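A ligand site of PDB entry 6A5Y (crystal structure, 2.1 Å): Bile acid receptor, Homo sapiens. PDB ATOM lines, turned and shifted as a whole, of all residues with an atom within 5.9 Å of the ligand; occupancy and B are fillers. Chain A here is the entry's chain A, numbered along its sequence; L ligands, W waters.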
ATOM      1  N   MET A  22       3.543  -5.974 -15.936  1.00  0.00           N
ATOM      2  CA  MET A  22       3.766  -6.846 -14.771  1.00  0.00           C
ATOM      3  C   MET A  22       5.091  -7.581 -15.048  1.00  0.00           C
ATOM      4  O   MET A  22       5.164  -8.256 -16.022  1.00  0.00           O
ATOM      5  CB  MET A  22       2.616  -7.842 -14.659  1.00  0.00           C
ATOM      6  CG  MET A  22       2.650  -8.823 -13.512  1.00  0.00           C
ATOM      7  SD  MET A  22       2.384  -8.065 -11.961  1.00  0.00           S
ATOM      8  CE  MET A  22       0.641  -7.618 -12.013  1.00  0.00           C
ATOM      9  N   THR A  27       5.066 -13.024 -12.933  1.00  0.00           N
ATOM     10  CA  THR A  27       4.130 -13.846 -13.741  1.00  0.00           C
ATOM     11  C   THR A  27       4.621 -15.305 -13.917  1.00  0.00           C
ATOM     12  O   THR A  27       3.782 -16.228 -13.986  1.00  0.00           O
ATOM     13  CB  THR A  27       3.846 -13.212 -15.095  1.00  0.00           C
ATOM     14  OG1 THR A  27       5.073 -13.059 -15.789  1.00  0.00           O
ATOM     15  CG2 THR A  27       3.204 -11.815 -14.891  1.00  0.00           C
ATOM     16  N   ILE A  30       3.089 -18.026 -11.652  1.00  0.00           N
ATOM     17  CA  ILE A  30       1.732 -18.545 -11.989  1.00  0.00           C
ATOM     18  C   ILE A  30       1.827 -20.075 -12.232  1.00  0.00           C
ATOM     19  O   ILE A  30       1.095 -20.837 -11.564  1.00  0.00           O
ATOM     20  CB  ILE A  30       1.135 -17.816 -13.210  1.00  0.00           C
ATOM     21  CG1 ILE A  30       0.802 -16.322 -12.812  1.00  0.00           C
ATOM     22  CG2 ILE A  30      -0.179 -18.500 -13.622  1.00  0.00           C
ATOM     23  CD1 ILE A  30       0.497 -15.431 -13.998  1.00  0.00           C
ATOM     24  N   PHE A  41      -2.135 -16.503  -2.310  1.00  0.00           N
ATOM     25  CA  PHE A  41      -2.169 -15.216  -1.638  1.00  0.00           C
ATOM     26  C   PHE A  41      -0.875 -14.392  -1.850  1.00  0.00           C
ATOM     27  O   PHE A  41      -0.955 -13.198  -2.097  1.00  0.00           O
ATOM     28  CB  PHE A  41      -2.534 -15.337  -0.134  1.00  0.00           C
ATOM     29  CG  PHE A  41      -2.564 -14.029   0.550  1.00  0.00           C
ATOM     30  CD1 PHE A  41      -3.687 -13.215   0.463  1.00  0.00           C
ATOM     31  CD2 PHE A  41      -1.431 -13.546   1.240  1.00  0.00           C
ATOM     32  CE1 PHE A  41      -3.700 -11.951   1.058  1.00  0.00           C
ATOM     33  CE2 PHE A  41      -1.426 -12.276   1.810  1.00  0.00           C
ATOM     34  CZ  PHE A  41      -2.583 -11.480   1.710  1.00  0.00           C
ATOM     35  N   LEU A  44      -0.655 -13.146  -5.473  1.00  0.00           N
ATOM     36  CA  LEU A  44      -1.585 -12.045  -5.664  1.00  0.00           C
ATOM     37  C   LEU A  44      -1.136 -10.736  -4.997  1.00  0.00           C
ATOM     38  O   LEU A  44      -1.263  -9.691  -5.590  1.00  0.00           O
ATOM     39  CB  LEU A  44      -2.976 -12.445  -5.126  1.00  0.00           C
ATOM     40  CG  LEU A  44      -3.678 -13.507  -5.985  1.00  0.00           C
ATOM     41  CD1 LEU A  44      -4.949 -13.948  -5.313  1.00  0.00           C
ATOM     42  CD2 LEU A  44      -3.964 -13.015  -7.390  1.00  0.00           C
ATOM     43  N   THR A  45      -0.657 -10.822  -3.774  1.00  0.00           N
ATOM     44  CA  THR A  45      -0.023  -9.693  -3.061  1.00  0.00           C
ATOM     45  C   THR A  45       1.127  -9.061  -3.862  1.00  0.00           C
ATOM     46  O   THR A  45       1.205  -7.827  -3.982  1.00  0.00           O
ATOM     47  CB  THR A  45       0.488 -10.191  -1.707  1.00  0.00           C
ATOM     48  OG1 THR A  45      -0.651 -10.441  -0.880  1.00  0.00           O
ATOM     49  CG2 THR A  45       1.360  -9.189  -1.036  1.00  0.00           C
ATOM     50  N   MET A  47       1.551  -9.313  -7.171  1.00  0.00           N
ATOM     51  CA  MET A  47       0.896  -8.664  -8.295  1.00  0.00           C
ATOM     52  C   MET A  47       0.207  -7.299  -7.957  1.00  0.00           C
ATOM     53  O   MET A  47       0.349  -6.326  -8.702  1.00  0.00           O
ATOM     54  CB  MET A  47      -0.161  -9.634  -8.856  1.00  0.00           C
ATOM     55  CG  MET A  47       0.422 -10.888  -9.507  1.00  0.00           C
ATOM     56  SD  MET A  47      -0.882 -12.034  -9.989  1.00  0.00           S
ATOM     57  CE  MET A  47       0.010 -12.962 -11.204  1.00  0.00           C
ATOM     58  N   ALA A  48      -0.561  -7.279  -6.895  1.00  0.00           N
ATOM     59  CA  ALA A  48      -1.246  -6.076  -6.380  1.00  0.00           C
ATOM     60  C   ALA A  48      -0.215  -4.950  -6.037  1.00  0.00           C
ATOM     61  O   ALA A  48      -0.360  -3.811  -6.436  1.00  0.00           O
ATOM     62  CB  ALA A  48      -2.069  -6.448  -5.156  1.00  0.00           C
ATOM     63  N   HIS A  51       1.075  -3.700  -9.229  1.00  0.00           N
ATOM     64  CA  HIS A  51       0.095  -2.981  -9.999  1.00  0.00           C
ATOM     65  C   HIS A  51      -0.258  -1.606  -9.358  1.00  0.00           C
ATOM     66  O   HIS A  51      -0.511  -0.667 -10.106  1.00  0.00           O
ATOM     67  CB  HIS A  51      -1.209  -3.765 -10.297  1.00  0.00           C
ATOM     68  CG  HIS A  51      -1.986  -3.117 -11.362  1.00  0.00           C
ATOM     69  ND1 HIS A  51      -1.484  -2.960 -12.630  1.00  0.00           N
ATOM     70  CD2 HIS A  51      -3.160  -2.426 -11.337  1.00  0.00           C
ATOM     71  CE1 HIS A  51      -2.323  -2.242 -13.356  1.00  0.00           C
ATOM     72  NE2 HIS A  51      -3.339  -1.883 -12.582  1.00  0.00           N
ATOM     73  N   ALA A  81      -8.331   2.962  -6.507  1.00  0.00           N
ATOM     74  CA  ALA A  81      -7.346   1.913  -6.758  1.00  0.00           C
ATOM     75  C   ALA A  81      -8.026   0.577  -6.957  1.00  0.00           C
ATOM     76  O   ALA A  81      -7.777  -0.115  -7.937  1.00  0.00           O
ATOM     77  CB  ALA A  81      -6.341   1.790  -5.618  1.00  0.00           C
ATOM     78  N   VAL A  82      -8.933   0.236  -6.057  1.00  0.00           N
ATOM     79  CA  VAL A  82      -9.610  -1.036  -6.160  1.00  0.00           C
ATOM     80  C   VAL A  82     -10.372  -1.190  -7.509  1.00  0.00           C
ATOM     81  O   VAL A  82     -10.215  -2.215  -8.226  1.00  0.00           O
ATOM     82  CB  VAL A  82     -10.548  -1.239  -4.987  1.00  0.00           C
ATOM     83  CG1 VAL A  82     -11.403  -2.495  -5.235  1.00  0.00           C
ATOM     84  CG2 VAL A  82      -9.759  -1.406  -3.694  1.00  0.00           C
ATOM     85  N   MET A  85      -8.072  -1.667 -10.376  1.00  0.00           N
ATOM     86  CA  MET A  85      -7.474  -2.997 -10.362  1.00  0.00           C
ATOM     87  C   MET A  85      -8.451  -4.084 -10.835  1.00  0.00           C
ATOM     88  O   MET A  85      -8.020  -4.997 -11.534  1.00  0.00           O
ATOM     89  CB  MET A  85      -6.885  -3.301  -8.983  1.00  0.00           C
ATOM     90  CG  MET A  85      -5.760  -2.315  -8.611  1.00  0.00           C
ATOM     91  SD  MET A  85      -5.288  -2.511  -6.883  1.00  0.00           S
ATOM     92  CE  MET A  85      -4.436  -4.062  -7.022  1.00  0.00           C
ATOM     93  N   PHE A  86      -9.738  -3.959 -10.507  1.00  0.00           N
ATOM     94  CA  PHE A  86     -10.761  -4.838 -11.046  1.00  0.00           C
ATOM     95  C   PHE A  86     -10.872  -4.683 -12.556  1.00  0.00           C
ATOM     96  O   PHE A  86     -10.956  -5.694 -13.239  1.00  0.00           O
ATOM     97  CB  PHE A  86     -12.176  -4.719 -10.359  1.00  0.00           C
ATOM     98  CG  PHE A  86     -12.288  -5.550  -9.091  1.00  0.00           C
ATOM     99  CD1 PHE A  86     -12.719  -6.885  -9.149  1.00  0.00           C
ATOM    100  CD2 PHE A  86     -11.906  -5.049  -7.847  1.00  0.00           C
ATOM    101  CE1 PHE A  86     -12.795  -7.655  -7.986  1.00  0.00           C
ATOM    102  CE2 PHE A  86     -11.945  -5.828  -6.681  1.00  0.00           C
ATOM    103  CZ  PHE A  86     -12.398  -7.134  -6.759  1.00  0.00           C
ATOM    104  N   ARG A  88      -8.534  -3.558 -14.601  1.00  0.00           N
ATOM    105  CA  ARG A  88      -7.307  -4.126 -15.168  1.00  0.00           C
ATOM    106  C   ARG A  88      -7.373  -5.660 -15.195  1.00  0.00           C
ATOM    107  O   ARG A  88      -7.092  -6.311 -16.250  1.00  0.00           O
ATOM    108  CB  ARG A  88      -6.083  -3.633 -14.399  1.00  0.00           C
ATOM    109  CG  ARG A  88      -4.765  -4.192 -14.887  1.00  0.00           C
ATOM    110  CD  ARG A  88      -4.449  -3.806 -16.288  1.00  0.00           C
ATOM    111  NE  ARG A  88      -3.121  -4.294 -16.635  1.00  0.00           N
ATOM    112  CZ  ARG A  88      -2.541  -4.162 -17.818  1.00  0.00           C
ATOM    113  NH1 ARG A  88      -3.133  -3.531 -18.831  1.00  0.00           N
ATOM    114  NH2 ARG A  88      -1.358  -4.677 -17.973  1.00  0.00           N
ATOM    115  N   SER A  89      -7.826  -6.238 -14.090  1.00  0.00           N
ATOM    116  CA  SER A  89      -8.000  -7.701 -14.086  1.00  0.00           C
ATOM    117  C   SER A  89      -8.973  -8.146 -15.155  1.00  0.00           C
ATOM    118  O   SER A  89      -8.724  -9.162 -15.793  1.00  0.00           O
ATOM    119  CB  SER A  89      -8.483  -8.270 -12.767  1.00  0.00           C
ATOM    120  OG  SER A  89      -7.533  -8.100 -11.775  1.00  0.00           O
ATOM    121  N   ILE A  92      -7.027  -8.137 -18.368  1.00  0.00           N
ATOM    122  CA  ILE A  92      -6.076  -9.310 -18.317  1.00  0.00           C
ATOM    123  C   ILE A  92      -6.751 -10.661 -18.610  1.00  0.00           C
ATOM    124  O   ILE A  92      -6.252 -11.487 -19.413  1.00  0.00           O
ATOM    125  CB  ILE A  92      -5.347  -9.360 -16.932  1.00  0.00           C
ATOM    126  CG1 ILE A  92      -4.307  -8.229 -16.823  1.00  0.00           C
ATOM    127  CG2 ILE A  92      -4.762 -10.745 -16.622  1.00  0.00           C
ATOM    128  CD1 ILE A  92      -3.395  -8.074 -17.995  1.00  0.00           C
ATOM    129  N   LEU A  97      -2.754 -14.330 -23.023  1.00  0.00           N
ATOM    130  CA  LEU A  97      -1.629 -14.312 -22.109  1.00  0.00           C
ATOM    131  C   LEU A  97      -0.711 -15.422 -22.567  1.00  0.00           C
ATOM    132  O   LEU A  97      -1.160 -16.257 -23.377  1.00  0.00           O
ATOM    133  CB  LEU A  97      -2.114 -14.611 -20.711  1.00  0.00           C
ATOM    134  CG  LEU A  97      -2.943 -13.456 -20.069  1.00  0.00           C
ATOM    135  CD1 LEU A  97      -3.287 -13.855 -18.635  1.00  0.00           C
ATOM    136  CD2 LEU A  97      -2.148 -12.170 -20.167  1.00  0.00           C
ATOM    137  N   PRO A  98       0.537 -15.477 -22.032  1.00  0.00           N
ATOM    138  CA  PRO A  98       1.408 -16.612 -22.336  1.00  0.00           C
ATOM    139  C   PRO A  98       0.730 -17.910 -21.976  1.00  0.00           C
ATOM    140  O   PRO A  98      -0.196 -17.924 -21.136  1.00  0.00           O
ATOM    141  CB  PRO A  98       2.644 -16.374 -21.480  1.00  0.00           C
ATOM    142  CG  PRO A  98       2.722 -14.904 -21.393  1.00  0.00           C
ATOM    143  CD  PRO A  98       1.262 -14.530 -21.171  1.00  0.00           C
ATOM    144  N   HIS A 101      -1.180 -19.167 -18.642  1.00  0.00           N
ATOM    145  CA  HIS A 101      -1.284 -18.094 -17.572  1.00  0.00           C
ATOM    146  C   HIS A 101      -2.742 -17.803 -17.175  1.00  0.00           C
ATOM    147  O   HIS A 101      -3.054 -17.844 -15.985  1.00  0.00           O
ATOM    148  CB  HIS A 101      -0.549 -16.820 -17.984  1.00  0.00           C
ATOM    149  CG  HIS A 101       0.938 -16.954 -17.933  1.00  0.00           C
ATOM    150  ND1 HIS A 101       1.768 -15.889 -17.667  1.00  0.00           N
ATOM    151  CD2 HIS A 101       1.740 -18.035 -18.072  1.00  0.00           C
ATOM    152  CE1 HIS A 101       3.026 -16.307 -17.656  1.00  0.00           C
ATOM    153  NE2 HIS A 101       3.032 -17.605 -17.909  1.00  0.00           N
ATOM    154  N   SER A 102      -3.622 -17.630 -18.160  1.00  0.00           N
ATOM    155  CA  SER A 102      -5.046 -17.384 -17.855  1.00  0.00           C
ATOM    156  C   SER A 102      -5.684 -18.428 -16.982  1.00  0.00           C
ATOM    157  O   SER A 102      -6.355 -18.080 -15.987  1.00  0.00           O
ATOM    158  CB  SER A 102      -5.931 -17.226 -19.100  1.00  0.00           C
ATOM    159  OG  SER A 102      -5.404 -16.283 -19.918  1.00  0.00           O
ATOM    160  N   LEU A 105      -3.870 -18.749 -13.465  1.00  0.00           N
ATOM    161  CA  LEU A 105      -4.127 -17.548 -12.588  1.00  0.00           C
ATOM    162  C   LEU A 105      -5.558 -17.591 -12.054  1.00  0.00           C
ATOM    163  O   LEU A 105      -5.811 -17.373 -10.880  1.00  0.00           O
ATOM    164  CB  LEU A 105      -3.838 -16.229 -13.349  1.00  0.00           C
ATOM    165  CG  LEU A 105      -4.144 -14.926 -12.601  1.00  0.00           C
ATOM    166  CD1 LEU A 105      -3.328 -14.882 -11.346  1.00  0.00           C
ATOM    167  CD2 LEU A 105      -3.903 -13.733 -13.527  1.00  0.00           C
ATOM    168  N   ILE A 109      -6.556 -17.651  -8.048  1.00  0.00           N
ATOM    169  CA  ILE A 109      -7.463 -16.633  -7.422  1.00  0.00           C
ATOM    170  C   ILE A 109      -8.645 -17.349  -6.782  1.00  0.00           C
ATOM    171  O   ILE A 109      -9.079 -16.965  -5.705  1.00  0.00           O
ATOM    172  CB  ILE A 109      -7.926 -15.648  -8.501  1.00  0.00           C
ATOM    173  CG1 ILE A 109      -6.742 -14.711  -8.824  1.00  0.00           C
ATOM    174  CG2 ILE A 109      -9.147 -14.861  -8.056  1.00  0.00           C
ATOM    175  CD1 ILE A 109      -7.009 -13.859 -10.016  1.00  0.00           C
ATOM    176  N   ILE A 114     -10.493 -16.395  -0.924  1.00  0.00           N
ATOM    177  CA  ILE A 114     -11.586 -15.442  -1.261  1.00  0.00           C
ATOM    178  C   ILE A 114     -12.790 -16.351  -1.269  1.00  0.00           C
ATOM    179  O   ILE A 114     -12.787 -17.423  -1.873  1.00  0.00           O
ATOM    180  CB  ILE A 114     -11.419 -14.792  -2.674  1.00  0.00           C
ATOM    181  CG1 ILE A 114     -10.157 -13.972  -2.748  1.00  0.00           C
ATOM    182  CG2 ILE A 114     -12.585 -13.884  -3.007  1.00  0.00           C
ATOM    183  CD1 ILE A 114      -9.670 -13.631  -4.146  1.00  0.00           C
ATOM    184  N   MET A 122     -16.986 -11.657  -9.268  1.00  0.00           N
ATOM    185  CA  MET A 122     -15.770 -11.134  -9.922  1.00  0.00           C
ATOM    186  C   MET A 122     -15.611 -11.695 -11.350  1.00  0.00           C
ATOM    187  O   MET A 122     -15.503 -10.919 -12.306  1.00  0.00           O
ATOM    188  CB  MET A 122     -14.564 -11.440  -9.010  1.00  0.00           C
ATOM    189  CG  MET A 122     -13.194 -11.301  -9.625  1.00  0.00           C
ATOM    190  SD  MET A 122     -11.872 -12.002  -8.581  1.00  0.00           S
ATOM    191  CE  MET A 122     -12.560 -11.488  -6.996  1.00  0.00           C
ATOM    192  N   TYR A 126     -15.899 -10.053 -15.172  1.00  0.00           N
ATOM    193  CA  TYR A 126     -14.884 -10.257 -16.230  1.00  0.00           C
ATOM    194  C   TYR A 126     -15.483 -10.724 -17.517  1.00  0.00           C
ATOM    195  O   TYR A 126     -15.133 -10.239 -18.606  1.00  0.00           O
ATOM    196  CB  TYR A 126     -13.699 -11.137 -15.826  1.00  0.00           C
ATOM    197  CG  TYR A 126     -12.933 -10.736 -14.547  1.00  0.00           C
ATOM    198  CD1 TYR A 126     -12.968  -9.443 -14.047  1.00  0.00           C
ATOM    199  CD2 TYR A 126     -12.227 -11.680 -13.846  1.00  0.00           C
ATOM    200  CE1 TYR A 126     -12.315  -9.135 -12.842  1.00  0.00           C
ATOM    201  CE2 TYR A 126     -11.529 -11.360 -12.677  1.00  0.00           C
ATOM    202  CZ  TYR A 126     -11.567 -10.074 -12.189  1.00  0.00           C
ATOM    203  OH  TYR A 126     -10.900  -9.788 -11.043  1.00  0.00           O
ATOM    204  N   HIS A 204     -14.449  -5.784  -1.894  1.00  0.00           N
ATOM    205  CA  HIS A 204     -13.026  -5.842  -1.591  1.00  0.00           C
ATOM    206  C   HIS A 204     -12.679  -5.614  -0.085  1.00  0.00           C
ATOM    207  O   HIS A 204     -11.800  -6.278   0.429  1.00  0.00           O
ATOM    208  CB  HIS A 204     -12.270  -4.884  -2.524  1.00  0.00           C
ATOM    209  CG  HIS A 204     -10.787  -5.032  -2.463  1.00  0.00           C
ATOM    210  ND1 HIS A 204     -10.020  -4.258  -1.656  1.00  0.00           N
ATOM    211  CD2 HIS A 204      -9.954  -5.869  -3.091  1.00  0.00           C
ATOM    212  CE1 HIS A 204      -8.759  -4.606  -1.796  1.00  0.00           C
ATOM    213  NE2 HIS A 204      -8.683  -5.578  -2.664  1.00  0.00           N
ATOM    214  N   MET A 207     -13.263  -8.967   1.485  1.00  0.00           N
ATOM    215  CA  MET A 207     -12.133  -9.847   1.179  1.00  0.00           C
ATOM    216  C   MET A 207     -10.904  -9.503   2.008  1.00  0.00           C
ATOM    217  O   MET A 207     -10.138 -10.373   2.472  1.00  0.00           O
ATOM    218  CB  MET A 207     -11.777  -9.683  -0.298  1.00  0.00           C
ATOM    219  CG  MET A 207     -12.755 -10.226  -1.291  1.00  0.00           C
ATOM    220  SD  MET A 207     -12.562  -9.579  -2.963  1.00  0.00           S
ATOM    221  CE  MET A 207     -10.881  -9.996  -3.366  1.00  0.00           C
ATOM    222  N   LEU A 208     -10.620  -8.222   2.181  1.00  0.00           N
ATOM    223  CA  LEU A 208      -9.440  -7.847   2.947  1.00  0.00           C
ATOM    224  C   LEU A 208      -9.572  -8.243   4.421  1.00  0.00           C
ATOM    225  O   LEU A 208      -8.588  -8.665   5.034  1.00  0.00           O
ATOM    226  CB  LEU A 208      -9.141  -6.356   2.842  1.00  0.00           C
ATOM    227  CG  LEU A 208      -8.697  -5.806   1.486  1.00  0.00           C
ATOM    228  CD1 LEU A 208      -8.582  -4.297   1.598  1.00  0.00           C
ATOM    229  CD2 LEU A 208      -7.380  -6.372   1.019  1.00  0.00           C
ATOM    230  N   TRP A 211      -9.143 -12.006   4.659  1.00  0.00           N
ATOM    231  CA  TRP A 211      -7.721 -12.300   4.603  1.00  0.00           C
ATOM    232  C   TRP A 211      -7.015 -11.995   5.904  1.00  0.00           C
ATOM    233  O   TRP A 211      -6.209 -12.796   6.393  1.00  0.00           O
ATOM    234  CB  TRP A 211      -7.073 -11.549   3.451  1.00  0.00           C
ATOM    235  CG  TRP A 211      -7.226 -12.255   2.120  1.00  0.00           C
ATOM    236  CD1 TRP A 211      -7.149 -13.577   1.895  1.00  0.00           C
ATOM    237  CD2 TRP A 211      -7.447 -11.646   0.856  1.00  0.00           C
ATOM    238  NE1 TRP A 211      -7.271 -13.831   0.586  1.00  0.00           N
ATOM    239  CE2 TRP A 211      -7.451 -12.656  -0.086  1.00  0.00           C
ATOM    240  CE3 TRP A 211      -7.557 -10.324   0.433  1.00  0.00           C
ATOM    241  CZ2 TRP A 211      -7.585 -12.399  -1.446  1.00  0.00           C
ATOM    242  CZ3 TRP A 211      -7.721 -10.059  -0.907  1.00  0.00           C
ATOM    243  CH2 TRP A 211      -7.721 -11.104  -1.846  1.00  0.00           C
ATOM    244  N   PHE A 218      -0.233  -7.955   4.484  1.00  0.00           N
ATOM    245  CA  PHE A 218      -0.076  -7.197   3.247  1.00  0.00           C
ATOM    246  C   PHE A 218       1.181  -6.341   3.288  1.00  0.00           C
ATOM    247  O   PHE A 218       1.606  -5.893   4.356  1.00  0.00           O
ATOM    248  CB  PHE A 218      -1.310  -6.313   3.006  1.00  0.00           C
ATOM    249  CG  PHE A 218      -2.615  -7.060   3.008  1.00  0.00           C
ATOM    250  CD1 PHE A 218      -3.110  -7.611   1.850  1.00  0.00           C
ATOM    251  CD2 PHE A 218      -3.342  -7.191   4.155  1.00  0.00           C
ATOM    252  CE1 PHE A 218      -4.313  -8.328   1.848  1.00  0.00           C
ATOM    253  CE2 PHE A 218      -4.548  -7.894   4.162  1.00  0.00           C
ATOM    254  CZ  PHE A 218      -5.018  -8.474   3.015  1.00  0.00           C
ATOM    255  N   LEU A 222       0.243  -1.577   0.179  1.00  0.00           N
ATOM    256  CA  LEU A 222      -1.150  -2.001   0.158  1.00  0.00           C
ATOM    257  C   LEU A 222      -1.878  -1.571   1.408  1.00  0.00           C
ATOM    258  O   LEU A 222      -3.083  -1.226   1.366  1.00  0.00           O
ATOM    259  CB  LEU A 222      -1.240  -3.533  -0.040  1.00  0.00           C
ATOM    260  CG  LEU A 222      -0.654  -4.047  -1.386  1.00  0.00           C
ATOM    261  CD1 LEU A 222      -0.813  -5.569  -1.505  1.00  0.00           C
ATOM    262  CD2 LEU A 222      -1.266  -3.352  -2.592  1.00  0.00           C
ATOM    263  N   TRP A 226      -5.111   0.962   0.811  1.00  0.00           N
ATOM    264  CA  TRP A 226      -6.405   0.386   1.156  1.00  0.00           C
ATOM    265  C   TRP A 226      -6.796   0.592   2.620  1.00  0.00           C
ATOM    266  O   TRP A 226      -7.760  -0.017   3.085  1.00  0.00           O
ATOM    267  CB  TRP A 226      -6.347  -1.120   0.875  1.00  0.00           C
ATOM    268  CG  TRP A 226      -6.246  -1.479  -0.569  1.00  0.00           C
ATOM    269  CD1 TRP A 226      -6.621  -0.726  -1.597  1.00  0.00           C
ATOM    270  CD2 TRP A 226      -5.724  -2.694  -1.116  1.00  0.00           C
ATOM    271  NE1 TRP A 226      -6.366  -1.369  -2.758  1.00  0.00           N
ATOM    272  CE2 TRP A 226      -5.813  -2.582  -2.497  1.00  0.00           C
ATOM    273  CE3 TRP A 226      -5.193  -3.862  -0.564  1.00  0.00           C
ATOM    274  CZ2 TRP A 226      -5.477  -3.611  -3.337  1.00  0.00           C
ATOM    275  CZ3 TRP A 226      -4.806  -4.880  -1.416  1.00  0.00           C
ATOM    276  CH2 TRP A 226      -4.966  -4.742  -2.784  1.00  0.00           C
HETATM  277  C1  LIG L   1      -8.816  -6.714  -8.157  1.00  0.00           C
HETATM  278  C2  LIG L   1      -8.099  -6.877  -6.989  1.00  0.00           C
HETATM  279  C3  LIG L   1      -7.830  -8.116  -6.474  1.00  0.00           C
HETATM  280  C4  LIG L   1      -8.223  -9.209  -7.233  1.00  0.00           C
HETATM  281  C5  LIG L   1      -8.912  -9.083  -8.420  1.00  0.00           C
HETATM  282  C6  LIG L   1      -9.188  -7.829  -8.875  1.00  0.00           C
HETATM  283  C7  LIG L   1      -6.972  -8.266  -5.294  1.00  0.00           C
HETATM  284  N1  LIG L   1      -7.373  -7.975  -4.062  1.00  0.00           N
HETATM  285  O1  LIG L   1      -6.271  -8.246  -3.191  1.00  0.00           O
HETATM  286  C8  LIG L   1      -5.233  -8.642  -3.966  1.00  0.00           C
HETATM  287  C9  LIG L   1      -5.651  -8.638  -5.259  1.00  0.00           C
HETATM  288  C10 LIG L   1      -3.957  -9.017  -3.336  1.00  0.00           C
HETATM  289  C11 LIG L   1      -3.995 -10.044  -2.227  1.00  0.00           C
HETATM  290  C12 LIG L   1      -3.709  -8.628  -1.905  1.00  0.00           C
HETATM  291  C13 LIG L   1      -4.923  -9.082  -6.433  1.00  0.00           C
HETATM  292  O2  LIG L   1      -4.331  -8.049  -7.153  1.00  0.00           O
HETATM  293  C14 LIG L   1      -4.575  -7.503  -8.424  1.00  0.00           C
HETATM  294  C15 LIG L   1      -3.352  -7.414  -9.332  1.00  0.00           C
HETATM  295  C16 LIG L   1      -4.228  -7.844 -10.547  1.00  0.00           C
HETATM  296  C17 LIG L   1      -5.295  -8.316  -9.491  1.00  0.00           C
HETATM  297  C18 LIG L   1      -3.642  -8.944 -11.415  1.00  0.00           C
HETATM  298  N2  LIG L   1      -2.897  -8.247 -12.452  1.00  0.00           N
HETATM  299  C19 LIG L   1      -3.129  -6.810 -12.378  1.00  0.00           C
HETATM  300  C20 LIG L   1      -4.418  -6.704 -11.565  1.00  0.00           C
HETATM  301  C21 LIG L   1      -2.201  -8.915 -13.461  1.00  0.00           C
HETATM  302  N3  LIG L   1      -1.651  -8.299 -14.498  1.00  0.00           N
HETATM  303  C22 LIG L   1      -1.041  -9.244 -15.329  1.00  0.00           C
HETATM  304  C23 LIG L   1      -1.155 -10.574 -14.897  1.00  0.00           C
HETATM  305  S1  LIG L   1      -2.071 -10.671 -13.438  1.00  0.00           S
HETATM  306  C24 LIG L   1      -0.339  -8.985 -16.511  1.00  0.00           C
HETATM  307  C25 LIG L   1       0.173 -10.066 -17.226  1.00  0.00           C
HETATM  308  C26 LIG L   1       0.047 -11.395 -16.767  1.00  0.00           C
HETATM  309  C27 LIG L   1      -0.611 -11.643 -15.578  1.00  0.00           C
HETATM  310  C28 LIG L   1       0.653 -12.595 -17.506  1.00  0.00           C
HETATM  311  O3  LIG L   1       1.204 -12.390 -18.564  1.00  0.00           O
HETATM  312  O4  LIG L   1       0.535 -13.712 -16.996  1.00  0.00           O
HETATM  313 CL1  LIG L   1      -7.620  -5.477  -6.097  1.00  0.00          CL
HETATM  314 CL2  LIG L   1      -7.933 -10.816  -6.667  1.00  0.00          CL
HETATM  315  O   HOH W   1       1.191 -10.812 -20.740  1.00  0.00           O
HETATM  316  O   HOH W   2      -1.344  -5.806 -15.293  1.00  0.00           O
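The side-chain hydroxyl of Tyr 126 sits close to the side-chain sulfur of Met 122 (3.5 Å).
The side-chain hydroxyl (OG1) of Thr 45 is in hydrogen-bond range of the backbone carbonyl oxygen (O) of Phe 41 (3.0 Å).
The backbone carbonyl oxygen of Met 85 lies within hydrogen-bond range of the side-chain hydroxyl of Ser 89, 3.2 Å away.
NE2 of His 204 is in hydrogen-bond range of N1 of the ligand (3.1 Å).
ND1 of His 101 sits at hydrogen-bond distance from O4 of the ligand, 2.6 Å away.
Water W2 lies within hydrogen-bond range of N3 of the ligand (2.6 Å) and NE of Arg 88 (2.7 Å).
Met 22 touches the ligand.
Thr 27 touches the ligand (CG2 to C26, 3.7 Å).
Ile 30 touches the ligand (CD1 to O4, 3.5 Å).
CE1 of Phe 41 touches C11 of the ligand (3.8 Å).
Leu 44 touches the ligand.
Thr 45 touches the ligand (OG1 to C11, 3.6 Å).
Met 47 touches the ligand (CE to S1, 3.8 Å).
Ala 48 touches the ligand (CB to O2, 3.4 Å).
His 51 touches the ligand.
Met 85 touches the ligand.
CD2 of Phe 86 touches C1 of the ligand, at 3.5 Å.
Arg 88 touches the ligand.
Ser 89 touches the ligand.
Ile 92 touches the ligand (CD1 to C24, 3.5 Å).
CD2 of Leu 97 touches O3 of the ligand, 3.7 Å away.
Pro 98 touches the ligand.
Leu 105 touches the ligand (CD2 to S1, 3.6 Å).
Tyr 126 touches the ligand.
Trp 211 touches the ligand.
CE1 of Phe 218 touches C12 of the ligand (3.8 Å).
Trp 226 touches the ligand (CH2 to O1, 3.8 Å).
Hydrophobic or aromatic side chains within 4 Å of the ligand: Met 22, Ile 30, Phe 41, Leu 44, Met 47, Ala 48, His 51, Met 85, Phe 86, Ile 92, Leu 97, Pro 98, His 101, Leu 105, His 204, Trp 211, Phe 218 and Trp 226.
Of the 32 residues printed, 23 come within 4 Å of the ligand.
The nearest printed residue that does not touch the ligand is Met 207 (4.1 Å).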
